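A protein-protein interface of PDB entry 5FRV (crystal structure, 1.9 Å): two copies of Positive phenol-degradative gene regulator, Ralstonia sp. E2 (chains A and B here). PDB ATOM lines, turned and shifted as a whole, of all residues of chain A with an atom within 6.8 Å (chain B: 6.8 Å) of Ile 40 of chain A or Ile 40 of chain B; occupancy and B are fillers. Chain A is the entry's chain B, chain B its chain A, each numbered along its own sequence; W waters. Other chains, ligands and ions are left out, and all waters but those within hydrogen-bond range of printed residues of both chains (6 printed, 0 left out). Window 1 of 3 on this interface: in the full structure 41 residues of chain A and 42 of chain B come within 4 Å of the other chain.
The backbone carbonyl oxygen of Glu 105 of chain B sits at hydrogen-bond distance from the backbone NH of Leu 41 of chain A, 2.9 Å away. O of Gly 106 of chain A sits at hydrogen-bond distance from NH2 of Arg 38 of chain B, 3.2 Å away. The backbone carbonyl oxygen of Gly 30 of chain B lies close to the backbone carbonyl oxygen of Gly 106 of chain A (3.3 Å). The backbone carbonyl oxygen (O) of Ile 40 of chain A sits close to the backbone carbonyl oxygen (O) of Ile 40 of chain B (3.3 Å). N of Leu 42 of chain B is in hydrogen-bond range of O of Ile 40 of chain A, 2.9 Å away. The backbone carbonyl oxygen (O) of Gly 106 of chain B lies close to the backbone carbonyl oxygen (O) of Gly 30 of chain A (3.2 Å). N of Leu 41 of chain B lies within hydrogen-bond range of O of Glu 105 of chain A, 2.8 Å away. O of Arg 38 of chain B is in hydrogen-bond range of N of Thr 44 of chain A (3.1 Å). NH2 of Arg 38 of chain A sits close to N of Phe 134 of chain B. The guanidinium group of Arg 38 of chain A sits at hydrogen-bond distance from the backbone carbonyl oxygen of Val 107 of chain B (3.4 Å). N of Ile 40 of chain B sits at hydrogen-bond distance from O of Leu 42 of chain A, 2.9 Å away. The backbone carbonyl oxygen of Arg 38 of chain A lies within hydrogen-bond range of the backbone NH of Thr 44 of chain B, at 3.1 Å. The guanidinium group (NH2) of Arg 38 of chain A lies within hydrogen-bond range of the backbone carbonyl oxygen (O) of Gly 106 of chain B, 3.2 Å away.
The backbone NH (N) of Phe 134 of chain A lies within hydrogen-bond range of the backbone carbonyl oxygen (O) of Val 107 of chain A, 3.0 Å away. The backbone carbonyl oxygen (O) of Ile 32 of chain A lies within hydrogen-bond range of the backbone NH (N) of Met 39 of chain A, 2.8 Å away. The guanidinium group (NH2) of Arg 38 of chain B lies within hydrogen-bond range of the backbone carbonyl oxygen (O) of Gly 30 of chain B. The guanidinium group (NH2) of Arg 38 of chain A sits at hydrogen-bond distance from the backbone carbonyl oxygen (O) of Gly 30 of chain A, 3.4 Å away. O of Ile 32 of chain B is in hydrogen-bond range of N of Met 39 of chain B (2.7 Å). O of Val 107 of chain B is in hydrogen-bond range of N of Phe 134 of chain B, 2.9 Å away.
Among the printed residues, pairs that only touch across the chains: Gly 30 of chain A with Val 107 of chain B (3.8 Å), Gly 30 of chain A with Val 108 of chain B (3.7 Å), Ile 32 of chain A with Glu 105 of chain B (3.5 Å), Ile 32 of chain A with Gly 106 of chain B (3.8 Å), Arg 38 of chain A with His 43 of chain B (3.7 Å), Met 39 of chain A with Leu 41 of chain B (3.9 Å), Met 39 of chain A with Leu 42 of chain B (3.3 Å), Met 39 of chain A with His 43 of chain B (3.4 Å), Ile 40 of chain A with Leu 41 of chain B (3.3 Å), Ile 40 of chain A with Thr 44 of chain B (3.8 Å), Ile 40 of chain A with Leu 47 of chain B (3.7 Å), Ile 40 of chain A with Glu 105 of chain B (3.4 Å), Ile 40 of chain A with Gly 106 of chain B (3.5 Å), Leu 41 of chain A with Ile 32 of chain B (3.9 Å), Leu 41 of chain A with Met 39 of chain B (3.9 Å), Leu 41 of chain A with Ile 40 of chain B (3.4 Å), Leu 41 of chain A with Leu 41 of chain B (3.6 Å), Leu 42 of chain A with Met 39 of chain B (3.2 Å), His 43 of chain A with Arg 38 of chain B (3.7 Å), His 43 of chain A with Met 39 of chain B (3.5 Å), His 43 of chain A with Glu 105 of chain B (3.6 Å), Thr 44 of chain A with Ile 40 of chain B (3.8 Å), Leu 47 of chain A with Ile 40 of chain B (3.6 Å), Glu 105 of chain A with Ile 32 of chain B (3.7 Å), Glu 105 of chain A with Ile 40 of chain B (3.4 Å), Glu 105 of chain A with His 43 of chain B (3.5 Å), Gly 106 of chain A with Ile 32 of chain B (3.98 Å), Gly 106 of chain A with Ile 40 of chain B (3.5 Å), Val 107 of chain A with Gly 30 of chain B (3.8 Å), Val 107 of chain A with Arg 38 of chain B (3.6 Å), Val 108 of chain A with Gly 30 of chain B (3.7 Å), Phe 134 of chain A with Arg 38 of chain B (3.6 Å) and Phe 134 of chain A with Ile 40 of chain B (3.9 Å).
Ile 40 of chain A touches seven residues of chain B. Of the printed residues of chain B, Leu 41 of chain A touches Ile 32 (3.9 Å), Met 39 (3.9 Å), Ile 40 (3.4 Å), Leu 41 (3.6 Å) and Glu 105 (2.9 Å). Of the printed residues of chain B, Gly 106 of chain A touches Gly 30, Ile 32, Arg 38 and Ile 40. Of the printed residues of chain B, Val 107 of chain A touches Gly 30 (3.8 Å) and Arg 38 (3.6 Å). Printed residues of chain A within 4 Å of Gly 30 of chain B: Gly 106 (3.2 Å), Val 107 (3.8 Å) and Val 108 (3.7 Å). Of chain A, only Ile 40, Leu 41, Leu 42, Thr 44, Leu 47, Glu 105, Gly 106 and Phe 134 come within 4 Å of Ile 40 of chain B. The nearest residue of chain B that does not touch Ile 40 of chain A is Phe 134 of chain B (4.05 Å). The nearest printed residue of chain B that does not touch Ile 32 of chain A is Leu 41 of chain B (4.2 Å).
Hydrophobic or aromatic side chains of chain B within 4 Å of the printed part of chain A: Ile 32, Met 39, Ile 40, Leu 41, His 43, Leu 47 and Phe 134. Hydrophobic or aromatic side chains of chain A within 4 Å of the printed part of chain B: Ile 32, Met 39, Ile 40, Leu 41, His 43, Leu 47 and Phe 134. Among the printed residues, no Asp or Glu carboxylate lies within 4 Å of a Lys or Arg side-chain nitrogen of the other chain.
Gly 30 of chain A touches Gly 106 of chain B, and with the chains exchanged Gly 106 of chain A touches Gly 30 of chain B. Arg 38 of chain A touches His 43 of chain B, and with the chains exchanged His 43 of chain A touches Arg 38 of chain B. Arg 38 of chain A touches Phe 134 of chain B, and with the chains exchanged Phe 134 of chain A touches Arg 38 of chain B. Leu 41 of chain A touches Glu 105 of chain B, and with the chains exchanged Glu 105 of chain A touches Leu 41 of chain B.
Water W1 lies within hydrogen-bond range of the backbone carbonyl oxygen of Met 39 of chain A (2.5 Å), the backbone carbonyl oxygen of Gly 106 of chain B (2.5 Å), the backbone NH of Ile 32 of chain A (2.9 Å) and the guanidinium group of Arg 38 of chain A (3.0 Å). Water W3 lies within hydrogen-bond range of the backbone carbonyl oxygen (O) of Met 39 of chain B, the backbone carbonyl oxygen (O) of Gly 106 of chain A, the guanidinium group (NE) of Arg 38 of chain B and the backbone NH (N) of Ile 32 of chain B. Water W2 bridges the backbone carbonyl oxygen (O) of Leu 41 of chain B (2.8 Å) and the side-chain carboxylate (OE1) of Glu 105 of chain A (2.9 Å). Water W6 bridges OE1 of Glu 105 of chain B (2.8 Å) and O of Leu 41 of chain A (2.8 Å). Water W4 lies within hydrogen-bond range of O of Arg 38 of chain B (3.0 Å) and N of Thr 44 of chain A (3.4 Å). Water W5 bridges O of Arg 38 of chain A (3.0 Å) and N of Thr 44 of chain B (3.3 Å).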
ATOM      1  N   GLY A  30      15.715 -16.966  14.997  1.00  0.00           N
ATOM      2  CA  GLY A  30      17.098 -16.871  15.459  1.00  0.00           C
ATOM      3  C   GLY A  30      18.100 -16.487  14.376  1.00  0.00           C
ATOM      4  O   GLY A  30      19.229 -16.980  14.353  1.00  0.00           O
ATOM      5  N   ILE A  32      19.805 -13.566  11.353  1.00  0.00           N
ATOM      6  CA  ILE A  32      20.118 -12.231  10.893  1.00  0.00           C
ATOM      7  C   ILE A  32      20.372 -12.315   9.402  1.00  0.00           C
ATOM      8  O   ILE A  32      21.099 -13.184   8.932  1.00  0.00           O
ATOM      9  CB  ILE A  32      21.354 -11.642  11.603  1.00  0.00           C
ATOM     10  CG1 ILE A  32      21.164 -11.647  13.118  1.00  0.00           C
ATOM     11  CG2 ILE A  32      21.620 -10.226  11.140  1.00  0.00           C
ATOM     12  CD1 ILE A  32      22.461 -11.383  13.887  1.00  0.00           C
ATOM     13  N   ARG A  38      22.453 -15.116   5.086  1.00  0.00           N
ATOM     14  CA  ARG A  38      22.391 -15.266   6.525  1.00  0.00           C
ATOM     15  C   ARG A  38      23.727 -14.841   7.135  1.00  0.00           C
ATOM     16  O   ARG A  38      24.790 -15.183   6.613  1.00  0.00           O
ATOM     17  CB  ARG A  38      22.049 -16.701   6.899  1.00  0.00           C
ATOM     18  CG  ARG A  38      21.774 -16.845   8.362  1.00  0.00           C
ATOM     19  CD  ARG A  38      21.162 -18.177   8.726  1.00  0.00           C
ATOM     20  NE  ARG A  38      21.097 -18.238  10.176  1.00  0.00           N
ATOM     21  CZ  ARG A  38      20.611 -19.254  10.874  1.00  0.00           C
ATOM     22  NH1 ARG A  38      20.115 -20.335  10.256  1.00  0.00           N
ATOM     23  NH2 ARG A  38      20.636 -19.181  12.195  1.00  0.00           N
ATOM     24  N   MET A  39      23.651 -14.076   8.218  1.00  0.00           N
ATOM     25  CA  MET A  39      24.835 -13.513   8.899  1.00  0.00           C
ATOM     26  C   MET A  39      24.856 -13.964  10.344  1.00  0.00           C
ATOM     27  O   MET A  39      23.797 -14.205  10.905  1.00  0.00           O
ATOM     28  CB  MET A  39      24.811 -11.979   8.859  1.00  0.00           C
ATOM     29  CG  MET A  39      24.490 -11.366   7.491  1.00  0.00           C
ATOM     30  SD  MET A  39      25.809 -11.652   6.314  1.00  0.00           S
ATOM     31  CE  MET A  39      26.999 -10.398   6.860  1.00  0.00           C
ATOM     32  N   ILE A  40      26.029 -14.050  10.978  1.00  0.00           N
ATOM     33  CA  ILE A  40      26.017 -14.088  12.442  1.00  0.00           C
ATOM     34  C   ILE A  40      26.828 -12.937  13.034  1.00  0.00           C
ATOM     35  O   ILE A  40      27.696 -12.346  12.385  1.00  0.00           O
ATOM     36  CB  ILE A  40      26.549 -15.435  13.031  1.00  0.00           C
ATOM     37  CG1 ILE A  40      28.004 -15.676  12.625  1.00  0.00           C
ATOM     38  CG2 ILE A  40      25.663 -16.614  12.602  1.00  0.00           C
ATOM     39  CD1 ILE A  40      28.650 -16.843  13.381  1.00  0.00           C
ATOM     40  N   LEU A  41      26.510 -12.590  14.267  1.00  0.00           N
ATOM     41  CA  LEU A  41      27.353 -11.679  15.010  1.00  0.00           C
ATOM     42  C   LEU A  41      28.364 -12.536  15.733  1.00  0.00           C
ATOM     43  O   LEU A  41      27.995 -13.420  16.510  1.00  0.00           O
ATOM     44  CB  LEU A  41      26.553 -10.827  15.996  1.00  0.00           C
ATOM     45  CG  LEU A  41      25.893  -9.585  15.405  1.00  0.00           C
ATOM     46  CD1 LEU A  41      24.744  -9.121  16.285  1.00  0.00           C
ATOM     47  CD2 LEU A  41      26.926  -8.449  15.185  1.00  0.00           C
ATOM     48  N   LEU A  42      29.640 -12.263  15.482  1.00  0.00           N
ATOM     49  CA  LEU A  42      30.715 -13.049  16.050  1.00  0.00           C
ATOM     50  C   LEU A  42      31.647 -12.110  16.795  1.00  0.00           C
ATOM     51  O   LEU A  42      31.900 -10.995  16.345  1.00  0.00           O
ATOM     52  CB  LEU A  42      31.464 -13.812  14.956  1.00  0.00           C
ATOM     53  CG  LEU A  42      32.503 -14.847  15.417  1.00  0.00           C
ATOM     54  CD1 LEU A  42      31.903 -15.872  16.371  1.00  0.00           C
ATOM     55  CD2 LEU A  42      33.099 -15.542  14.200  1.00  0.00           C
ATOM     56  N   HIS A  43      32.095 -12.560  17.963  1.00  0.00           N
ATOM     57  CA  HIS A  43      33.083 -11.827  18.762  1.00  0.00           C
ATOM     58  C   HIS A  43      34.421 -11.787  18.056  1.00  0.00           C
ATOM     59  O   HIS A  43      34.964 -12.844  17.720  1.00  0.00           O
ATOM     60  CB  HIS A  43      33.239 -12.495  20.141  1.00  0.00           C
ATOM     61  CG  HIS A  43      31.942 -12.688  20.863  1.00  0.00           C
ATOM     62  ND1 HIS A  43      31.028 -13.658  20.505  1.00  0.00           N
ATOM     63  CD2 HIS A  43      31.400 -12.022  21.909  1.00  0.00           C
ATOM     64  CE1 HIS A  43      29.972 -13.572  21.296  1.00  0.00           C
ATOM     65  NE2 HIS A  43      30.183 -12.605  22.172  1.00  0.00           N
ATOM     66  N   THR A  44      34.975 -10.596  17.843  1.00  0.00           N
ATOM     67  CA  THR A  44      36.310 -10.516  17.254  1.00  0.00           C
ATOM     68  C   THR A  44      37.348 -11.243  18.105  1.00  0.00           C
ATOM     69  O   THR A  44      38.314 -11.787  17.557  1.00  0.00           O
ATOM     70  CB  THR A  44      36.751  -9.054  17.006  1.00  0.00           C
ATOM     71  OG1 THR A  44      36.803  -8.333  18.239  1.00  0.00           O
ATOM     72  CG2 THR A  44      35.757  -8.384  16.081  1.00  0.00           C
ATOM     73  N   LEU A  47      37.167 -14.874  16.969  1.00  0.00           N
ATOM     74  CA  LEU A  47      37.820 -15.003  15.674  1.00  0.00           C
ATOM     75  C   LEU A  47      39.320 -14.831  15.869  1.00  0.00           C
ATOM     76  O   LEU A  47      40.125 -15.519  15.239  1.00  0.00           O
ATOM     77  CB  LEU A  47      37.261 -13.970  14.669  1.00  0.00           C
ATOM     78  CG  LEU A  47      36.561 -14.461  13.406  1.00  0.00           C
ATOM     79  CD1 LEU A  47      36.317 -13.306  12.426  1.00  0.00           C
ATOM     80  CD2 LEU A  47      37.303 -15.605  12.710  1.00  0.00           C
ATOM     81  N   GLU A 105      29.055  -4.038   8.416  1.00  0.00           N
ATOM     82  CA  GLU A 105      29.361  -5.337   9.024  1.00  0.00           C
ATOM     83  C   GLU A 105      30.275  -5.206  10.247  1.00  0.00           C
ATOM     84  O   GLU A 105      30.495  -6.188  10.969  1.00  0.00           O
ATOM     85  CB  GLU A 105      29.968  -6.259   7.971  1.00  0.00           C
ATOM     86  CG  GLU A 105      28.855  -6.780   6.990  1.00  0.00           C
ATOM     87  CD  GLU A 105      29.386  -7.242   5.643  1.00  0.00           C
ATOM     88  OE1 GLU A 105      30.614  -7.428   5.506  1.00  0.00           O
ATOM     89  OE2 GLU A 105      28.568  -7.407   4.705  1.00  0.00           O
ATOM     90  N   GLY A 106      30.784  -3.991  10.488  1.00  0.00           N
ATOM     91  CA  GLY A 106      31.613  -3.718  11.654  1.00  0.00           C
ATOM     92  C   GLY A 106      33.032  -4.189  11.446  1.00  0.00           C
ATOM     93  O   GLY A 106      33.802  -4.336  12.393  1.00  0.00           O
ATOM     94  N   VAL A 107      33.389  -4.457  10.199  1.00  0.00           N
ATOM     95  CA  VAL A 107      34.693  -5.034   9.948  1.00  0.00           C
ATOM     96  C   VAL A 107      35.765  -3.926   9.989  1.00  0.00           C
ATOM     97  O   VAL A 107      36.814  -4.095  10.615  1.00  0.00           O
ATOM     98  CB  VAL A 107      34.717  -5.789   8.613  1.00  0.00           C
ATOM     99  CG1 VAL A 107      36.119  -6.198   8.282  1.00  0.00           C
ATOM    100  CG2 VAL A 107      33.788  -7.052   8.677  1.00  0.00           C
ATOM    101  N   VAL A 108      35.458  -2.782   9.378  1.00  0.00           N
ATOM    102  CA  VAL A 108      36.404  -1.665   9.235  1.00  0.00           C
ATOM    103  C   VAL A 108      35.624  -0.443   8.787  1.00  0.00           C
ATOM    104  O   VAL A 108      34.590  -0.585   8.142  1.00  0.00           O
ATOM    105  CB  VAL A 108      37.506  -1.998   8.222  1.00  0.00           C
ATOM    106  CG1 VAL A 108      36.880  -2.341   6.847  1.00  0.00           C
ATOM    107  CG2 VAL A 108      38.508  -0.867   8.089  1.00  0.00           C
ATOM    108  N   PHE A 134      39.292  -4.220  12.358  1.00  0.00           N
ATOM    109  CA  PHE A 134      39.163  -5.167  13.464  1.00  0.00           C
ATOM    110  C   PHE A 134      40.309  -6.157  13.396  1.00  0.00           C
ATOM    111  O   PHE A 134      40.827  -6.599  14.421  1.00  0.00           O
ATOM    112  CB  PHE A 134      37.816  -5.912  13.443  1.00  0.00           C
ATOM    113  CG  PHE A 134      37.867  -7.259  12.771  1.00  0.00           C
ATOM    114  CD1 PHE A 134      38.152  -8.401  13.511  1.00  0.00           C
ATOM    115  CD2 PHE A 134      37.608  -7.387  11.414  1.00  0.00           C
ATOM    116  CE1 PHE A 134      38.203  -9.657  12.911  1.00  0.00           C
ATOM    117  CE2 PHE A 134      37.648  -8.636  10.798  1.00  0.00           C
ATOM    118  CZ  PHE A 134      37.939  -9.776  11.562  1.00  0.00           C
ATOM    119  N   MET A 153      41.599 -11.102   5.874  1.00  0.00           N
ATOM    120  CA  MET A 153      40.198 -11.307   5.515  1.00  0.00           C
ATOM    121  C   MET A 153      39.610 -10.035   4.920  1.00  0.00           C
ATOM    122  O   MET A 153      38.779 -10.085   4.007  1.00  0.00           O
ATOM    123  CB  MET A 153      39.402 -11.778   6.741  1.00  0.00           C
ATOM    124  CG  MET A 153      37.899 -11.883   6.545  1.00  0.00           C
ATOM    125  SD  MET A 153      37.084 -12.461   8.066  1.00  0.00           S
ATOM    126  CE  MET A 153      38.364 -12.259   9.280  1.00  0.00           C
ATOM    127  N   GLY B  30      32.604   2.298  11.915  1.00  0.00           N
ATOM    128  CA  GLY B  30      32.653   1.000  11.262  1.00  0.00           C
ATOM    129  C   GLY B  30      32.753  -0.137  12.264  1.00  0.00           C
ATOM    130  O   GLY B  30      33.460  -1.122  12.028  1.00  0.00           O
ATOM    131  N   ILE B  32      30.783  -2.548  15.687  1.00  0.00           N
ATOM    132  CA  ILE B  32      29.611  -3.065  16.368  1.00  0.00           C
ATOM    133  C   ILE B  32      30.067  -3.599  17.715  1.00  0.00           C
ATOM    134  O   ILE B  32      31.042  -4.339  17.765  1.00  0.00           O
ATOM    135  CB  ILE B  32      28.944  -4.210  15.588  1.00  0.00           C
ATOM    136  CG1 ILE B  32      28.532  -3.768  14.178  1.00  0.00           C
ATOM    137  CG2 ILE B  32      27.750  -4.784  16.363  1.00  0.00           C
ATOM    138  CD1 ILE B  32      27.942  -4.922  13.382  1.00  0.00           C
ATOM    139  N   ARG B  38      33.730  -6.216  21.028  1.00  0.00           N
ATOM    140  CA  ARG B  38      33.540  -5.829  19.663  1.00  0.00           C
ATOM    141  C   ARG B  38      33.107  -7.042  18.865  1.00  0.00           C
ATOM    142  O   ARG B  38      33.602  -8.158  19.091  1.00  0.00           O
ATOM    143  CB  ARG B  38      34.818  -5.235  19.106  1.00  0.00           C
ATOM    144  CG  ARG B  38      34.663  -4.780  17.679  1.00  0.00           C
ATOM    145  CD  ARG B  38      35.856  -4.003  17.157  1.00  0.00           C
ATOM    146  NE  ARG B  38      35.579  -3.569  15.788  1.00  0.00           N
ATOM    147  CZ  ARG B  38      36.433  -2.928  14.999  1.00  0.00           C
ATOM    148  NH1 ARG B  38      37.661  -2.619  15.429  1.00  0.00           N
ATOM    149  NH2 ARG B  38      36.051  -2.599  13.776  1.00  0.00           N
ATOM    150  N   MET B  39      32.165  -6.826  17.946  1.00  0.00           N
ATOM    151  CA  MET B  39      31.602  -7.903  17.121  1.00  0.00           C
ATOM    152  C   MET B  39      31.783  -7.578  15.632  1.00  0.00           C
ATOM    153  O   MET B  39      31.919  -6.416  15.282  1.00  0.00           O
ATOM    154  CB  MET B  39      30.109  -8.081  17.406  1.00  0.00           C
ATOM    155  CG  MET B  39      29.734  -8.032  18.877  1.00  0.00           C
ATOM    156  SD  MET B  39      30.263  -9.485  19.783  1.00  0.00           S
ATOM    157  CE  MET B  39      29.036 -10.654  19.170  1.00  0.00           C
ATOM    158  N   ILE B  40      31.765  -8.594  14.763  1.00  0.00           N
ATOM    159  CA  ILE B  40      31.540  -8.371  13.336  1.00  0.00           C
ATOM    160  C   ILE B  40      30.355  -9.209  12.860  1.00  0.00           C
ATOM    161  O   ILE B  40      30.031 -10.261  13.445  1.00  0.00           O
ATOM    162  CB  ILE B  40      32.780  -8.721  12.445  1.00  0.00           C
ATOM    163  CG1 ILE B  40      33.144 -10.206  12.561  1.00  0.00           C
ATOM    164  CG2 ILE B  40      33.995  -7.821  12.783  1.00  0.00           C
ATOM    165  CD1 ILE B  40      34.063 -10.690  11.441  1.00  0.00           C
ATOM    166  N   LEU B  41      29.684  -8.713  11.824  1.00  0.00           N
ATOM    167  CA  LEU B  41      28.680  -9.515  11.102  1.00  0.00           C
ATOM    168  C   LEU B  41      29.411 -10.312  10.062  1.00  0.00           C
ATOM    169  O   LEU B  41      30.076  -9.733   9.194  1.00  0.00           O
ATOM    170  CB  LEU B  41      27.617  -8.641  10.434  1.00  0.00           C
ATOM    171  CG  LEU B  41      26.533  -8.037  11.322  1.00  0.00           C
ATOM    172  CD1 LEU B  41      25.748  -6.948  10.598  1.00  0.00           C
ATOM    173  CD2 LEU B  41      25.622  -9.160  11.796  1.00  0.00           C
ATOM    174  N   LEU B  42      29.292 -11.631  10.130  1.00  0.00           N
ATOM    175  CA  LEU B  42      30.005 -12.503   9.202  1.00  0.00           C
ATOM    176  C   LEU B  42      29.034 -13.376   8.420  1.00  0.00           C
ATOM    177  O   LEU B  42      28.150 -13.956   9.025  1.00  0.00           O
ATOM    178  CB  LEU B  42      30.976 -13.403   9.962  1.00  0.00           C
ATOM    179  CG  LEU B  42      32.017 -14.207   9.183  1.00  0.00           C
ATOM    180  CD1 LEU B  42      32.884 -13.293   8.327  1.00  0.00           C
ATOM    181  CD2 LEU B  42      32.880 -14.966  10.171  1.00  0.00           C
ATOM    182  N   HIS B  43      29.236 -13.509   7.106  1.00  0.00           N
ATOM    183  CA  HIS B  43      28.391 -14.413   6.297  1.00  0.00           C
ATOM    184  C   HIS B  43      28.580 -15.871   6.723  1.00  0.00           C
ATOM    185  O   HIS B  43      29.710 -16.366   6.789  1.00  0.00           O
ATOM    186  CB  HIS B  43      28.713 -14.266   4.807  1.00  0.00           C
ATOM    187  CG  HIS B  43      28.686 -12.851   4.324  1.00  0.00           C
ATOM    188  ND1 HIS B  43      29.666 -11.931   4.646  1.00  0.00           N
ATOM    189  CD2 HIS B  43      27.790 -12.191   3.555  1.00  0.00           C
ATOM    190  CE1 HIS B  43      29.373 -10.770   4.093  1.00  0.00           C
ATOM    191  NE2 HIS B  43      28.243 -10.903   3.424  1.00  0.00           N
ATOM    192  N   THR B  44      27.488 -16.558   7.047  1.00  0.00           N
ATOM    193  CA  THR B  44      27.609 -17.974   7.386  1.00  0.00           C
ATOM    194  C   THR B  44      28.238 -18.762   6.222  1.00  0.00           C
ATOM    195  O   THR B  44      28.923 -19.764   6.444  1.00  0.00           O
ATOM    196  CB  THR B  44      26.254 -18.578   7.760  1.00  0.00           C
ATOM    197  OG1 THR B  44      25.364 -18.471   6.642  1.00  0.00           O
ATOM    198  CG2 THR B  44      25.668 -17.828   8.957  1.00  0.00           C
ATOM    199  N   LEU B  47      31.867 -18.538   6.703  1.00  0.00           N
ATOM    200  CA  LEU B  47      32.290 -19.442   7.773  1.00  0.00           C
ATOM    201  C   LEU B  47      32.231 -20.877   7.256  1.00  0.00           C
ATOM    202  O   LEU B  47      33.072 -21.703   7.602  1.00  0.00           O
ATOM    203  CB  LEU B  47      31.429 -19.291   9.024  1.00  0.00           C
ATOM    204  CG  LEU B  47      32.029 -18.481  10.184  1.00  0.00           C
ATOM    205  CD1 LEU B  47      31.180 -18.614  11.411  1.00  0.00           C
ATOM    206  CD2 LEU B  47      33.472 -18.855  10.496  1.00  0.00           C
ATOM    207  N   GLU B 105      22.530 -13.046  18.404  1.00  0.00           N
ATOM    208  CA  GLU B 105      23.701 -13.144  17.525  1.00  0.00           C
ATOM    209  C   GLU B 105      23.392 -13.914  16.260  1.00  0.00           C
ATOM    210  O   GLU B 105      24.242 -14.028  15.361  1.00  0.00           O
ATOM    211  CB  GLU B 105      24.895 -13.780  18.264  1.00  0.00           C
ATOM    212  CG  GLU B 105      25.402 -12.872  19.384  1.00  0.00           C
ATOM    213  CD  GLU B 105      26.189 -13.590  20.462  1.00  0.00           C
ATOM    214  OE1 GLU B 105      26.513 -14.799  20.334  1.00  0.00           O
ATOM    215  OE2 GLU B 105      26.452 -12.933  21.473  1.00  0.00           O
ATOM    216  N   GLY B 106      22.155 -14.399  16.154  1.00  0.00           N
ATOM    217  CA  GLY B 106      21.689 -15.024  14.920  1.00  0.00           C
ATOM    218  C   GLY B 106      22.268 -16.406  14.675  1.00  0.00           C
ATOM    219  O   GLY B 106      22.329 -16.886  13.541  1.00  0.00           O
ATOM    220  N   VAL B 107      22.720 -17.041  15.747  1.00  0.00           N
ATOM    221  CA  VAL B 107      23.378 -18.333  15.646  1.00  0.00           C
ATOM    222  C   VAL B 107      22.322 -19.453  15.572  1.00  0.00           C
ATOM    223  O   VAL B 107      22.437 -20.397  14.779  1.00  0.00           O
ATOM    224  CB  VAL B 107      24.362 -18.498  16.835  1.00  0.00           C
ATOM    225  CG1 VAL B 107      24.875 -19.923  16.979  1.00  0.00           C
ATOM    226  CG2 VAL B 107      25.548 -17.506  16.676  1.00  0.00           C
ATOM    227  N   VAL B 108      21.269 -19.306  16.369  1.00  0.00           N
ATOM    228  CA  VAL B 108      20.260 -20.345  16.554  1.00  0.00           C
ATOM    229  C   VAL B 108      19.122 -19.754  17.384  1.00  0.00           C
ATOM    230  O   VAL B 108      19.321 -18.785  18.125  1.00  0.00           O
ATOM    231  CB  VAL B 108      20.845 -21.632  17.244  1.00  0.00           C
ATOM    232  CG1 VAL B 108      21.440 -21.324  18.622  1.00  0.00           C
ATOM    233  CG2 VAL B 108      19.790 -22.749  17.376  1.00  0.00           C
ATOM    234  N   PHE B 134      22.305 -22.202  12.539  1.00  0.00           N
ATOM    235  CA  PHE B 134      23.038 -21.843  11.338  1.00  0.00           C
ATOM    236  C   PHE B 134      24.057 -22.921  11.026  1.00  0.00           C
ATOM    237  O   PHE B 134      24.315 -23.236   9.871  1.00  0.00           O
ATOM    238  CB  PHE B 134      23.740 -20.485  11.484  1.00  0.00           C
ATOM    239  CG  PHE B 134      25.172 -20.580  11.952  1.00  0.00           C
ATOM    240  CD1 PHE B 134      25.472 -20.596  13.302  1.00  0.00           C
ATOM    241  CD2 PHE B 134      26.217 -20.652  11.036  1.00  0.00           C
ATOM    242  CE1 PHE B 134      26.780 -20.685  13.731  1.00  0.00           C
ATOM    243  CE2 PHE B 134      27.519 -20.756  11.452  1.00  0.00           C
ATOM    244  CZ  PHE B 134      27.807 -20.767  12.803  1.00  0.00           C
ATOM    245  N   MET B 153      30.541 -25.118  17.106  1.00  0.00           N
ATOM    246  CA  MET B 153      30.649 -23.794  17.714  1.00  0.00           C
ATOM    247  C   MET B 153      29.484 -23.538  18.643  1.00  0.00           C
ATOM    248  O   MET B 153      29.657 -22.914  19.688  1.00  0.00           O
ATOM    249  CB  MET B 153      30.706 -22.700  16.643  1.00  0.00           C
ATOM    250  CG  MET B 153      31.156 -21.332  17.131  1.00  0.00           C
ATOM    251  SD  MET B 153      31.090 -20.153  15.707  1.00  0.00           S
ATOM    252  CE  MET B 153      31.216 -21.285  14.369  1.00  0.00           C
HETATM  253  O   HOH W   1      21.858 -15.658  11.423  1.00  0.00           O
HETATM  254  O   HOH W   2      31.731  -9.650   6.999  1.00  0.00           O
HETATM  255  O   HOH W   3      33.118  -4.240  14.947  1.00  0.00           O
HETATM  256  O   HOH W   4      35.153  -9.726  21.086  1.00  0.00           O
HETATM  257  O   HOH W   5      25.998 -16.218   4.087  1.00  0.00           O
HETATM  258  O   HOH W   6      28.274 -15.526  18.326  1.00  0.00           O
